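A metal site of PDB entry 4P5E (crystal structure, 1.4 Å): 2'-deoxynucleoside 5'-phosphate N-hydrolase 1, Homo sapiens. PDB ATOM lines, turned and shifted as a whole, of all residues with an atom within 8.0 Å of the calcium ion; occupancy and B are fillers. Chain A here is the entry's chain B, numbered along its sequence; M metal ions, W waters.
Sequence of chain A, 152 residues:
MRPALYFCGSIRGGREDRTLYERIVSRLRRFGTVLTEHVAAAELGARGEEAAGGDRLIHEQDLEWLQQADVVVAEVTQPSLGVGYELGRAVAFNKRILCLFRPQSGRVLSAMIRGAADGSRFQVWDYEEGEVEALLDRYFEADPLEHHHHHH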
ATOM      1  N   ARG A  96      16.147 -25.149 -23.675  1.00  0.00           N
ATOM      2  CA  ARG A  96      16.817 -24.883 -22.408  1.00  0.00           C
ATOM      3  C   ARG A  96      17.470 -26.184 -21.935  1.00  0.00           C
ATOM      4  O   ARG A  96      16.789 -27.195 -21.812  1.00  0.00           O
ATOM      5  CB  ARG A  96      15.810 -24.367 -21.394  1.00  0.00           C
ATOM      6  CG  ARG A  96      16.388 -24.164 -20.024  1.00  0.00           C
ATOM      7  CD  ARG A  96      15.298 -23.669 -19.100  1.00  0.00           C
ATOM      8  NE  ARG A  96      15.737 -23.665 -17.715  1.00  0.00           N
ATOM      9  CZ  ARG A  96      15.011 -23.190 -16.716  1.00  0.00           C
ATOM     10  NH1 ARG A  96      13.805 -22.691 -16.951  1.00  0.00           N
ATOM     11  NH2 ARG A  96      15.471 -23.216 -15.470  1.00  0.00           N
ATOM     12  N   PHE A 140      15.789 -24.435 -10.774  1.00  0.00           N
ATOM     13  CA  PHE A 140      14.405 -24.134 -11.134  1.00  0.00           C
ATOM     14  C   PHE A 140      13.811 -22.992 -10.311  1.00  0.00           C
ATOM     15  O   PHE A 140      12.882 -22.329 -10.776  1.00  0.00           O
ATOM     16  CB  PHE A 140      13.578 -25.428 -11.059  1.00  0.00           C
ATOM     17  CG  PHE A 140      13.876 -26.373 -12.197  1.00  0.00           C
ATOM     18  CD1 PHE A 140      13.576 -26.004 -13.513  1.00  0.00           C
ATOM     19  CD2 PHE A 140      14.515 -27.586 -11.978  1.00  0.00           C
ATOM     20  CE1 PHE A 140      13.872 -26.865 -14.589  1.00  0.00           C
ATOM     21  CE2 PHE A 140      14.801 -28.427 -13.044  1.00  0.00           C
ATOM     22  CZ  PHE A 140      14.480 -28.060 -14.348  1.00  0.00           C
ATOM     23  N   ALA A 142      15.560 -20.256  -9.655  1.00  0.00           N
ATOM     24  CA  ALA A 142      16.128 -19.090 -10.362  1.00  0.00           C
ATOM     25  C   ALA A 142      15.373 -18.763 -11.663  1.00  0.00           C
ATOM     26  O   ALA A 142      15.205 -17.600 -12.003  1.00  0.00           O
ATOM     27  CB  ALA A 142      17.604 -19.329 -10.666  1.00  0.00           C
ATOM     28  N   ASP A 143      14.928 -19.797 -12.382  1.00  0.00           N
ATOM     29  CA  ASP A 143      14.097 -19.654 -13.589  1.00  0.00           C
ATOM     30  C   ASP A 143      13.044 -20.743 -13.606  1.00  0.00           C
ATOM     31  O   ASP A 143      13.274 -21.818 -14.152  1.00  0.00           O
ATOM     32  CB  ASP A 143      14.944 -19.689 -14.871  1.00  0.00           C
ATOM     33  CG  ASP A 143      14.127 -19.370 -16.158  1.00  0.00           C
ATOM     34  OD1 ASP A 143      12.880 -19.385 -16.149  1.00  0.00           O
ATOM     35  OD2 ASP A 143      14.762 -19.121 -17.202  1.00  0.00           O
ATOM     36  N   PRO A 144      11.875 -20.483 -13.011  1.00  0.00           N
ATOM     37  CA  PRO A 144      10.826 -21.512 -12.947  1.00  0.00           C
ATOM     38  C   PRO A 144      10.300 -21.945 -14.317  1.00  0.00           C
ATOM     39  O   PRO A 144      10.302 -21.156 -15.242  1.00  0.00           O
ATOM     40  CB  PRO A 144       9.723 -20.836 -12.134  1.00  0.00           C
ATOM     41  CG  PRO A 144      10.434 -19.771 -11.335  1.00  0.00           C
ATOM     42  CD  PRO A 144      11.518 -19.275 -12.235  1.00  0.00           C
ATOM     43  N   LEU A 145       9.891 -23.209 -14.414  1.00  0.00           N
ATOM     44  CA  LEU A 145       9.090 -23.694 -15.538  1.00  0.00           C
ATOM     45  C   LEU A 145       7.628 -23.403 -15.246  1.00  0.00           C
ATOM     46  O   LEU A 145       7.118 -23.825 -14.216  1.00  0.00           O
ATOM     47  CB  LEU A 145       9.233 -25.193 -15.724  1.00  0.00           C
ATOM     48  CG  LEU A 145      10.584 -25.814 -16.039  1.00  0.00           C
ATOM     49  CD1 LEU A 145      10.428 -27.327 -16.033  1.00  0.00           C
ATOM     50  CD2 LEU A 145      11.094 -25.318 -17.374  1.00  0.00           C
ATOM     51  N   GLU A 146       6.950 -22.696 -16.140  1.00  0.00           N
ATOM     52  CA  GLU A 146       5.562 -22.340 -15.868  1.00  0.00           C
ATOM     53  C   GLU A 146       4.556 -23.195 -16.642  1.00  0.00           C
ATOM     54  O   GLU A 146       4.919 -23.964 -17.533  1.00  0.00           O
ATOM     55  CB  GLU A 146       5.334 -20.856 -16.187  1.00  0.00           C
ATOM     56  CG  GLU A 146       6.198 -19.915 -15.349  1.00  0.00           C
ATOM     57  CD  GLU A 146       7.428 -19.423 -16.099  1.00  0.00           C
ATOM     58  OE1 GLU A 146       8.099 -18.501 -15.584  1.00  0.00           O
ATOM     59  OE2 GLU A 146       7.717 -19.968 -17.186  1.00  0.00           O
HETATM   60 CA    CA M   1      10.336 -19.274 -16.641  1.00  0.00          CA
HETATM   61  O   HOH W   1      10.887 -17.460 -15.323  1.00  0.00           O
HETATM   62  O   HOH W   2      10.325 -20.629 -18.529  1.00  0.00           O
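Water W1 binds the calcium ion (2.3 Å).
Water W2 is bound to the calcium ion (2.3 Å).
The calcium ion is bound by O of Pro 144 (2.3 Å).
The side-chain carboxylate (OE1) of Glu 146 is bound to the calcium ion.
The calcium ion is bound by OD1 of Asp 143.
OE2 of Glu 146 is bound to the calcium ion (2.8 Å).
The guanidinium group (NH1) of Arg 96 is in salt-bridge range of the side-chain carboxylate (OD2) of Asp 143, at 3.7 Å.
The nearest printed residue that does not touch the calcium ion is Leu 145 (4.5 Å).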
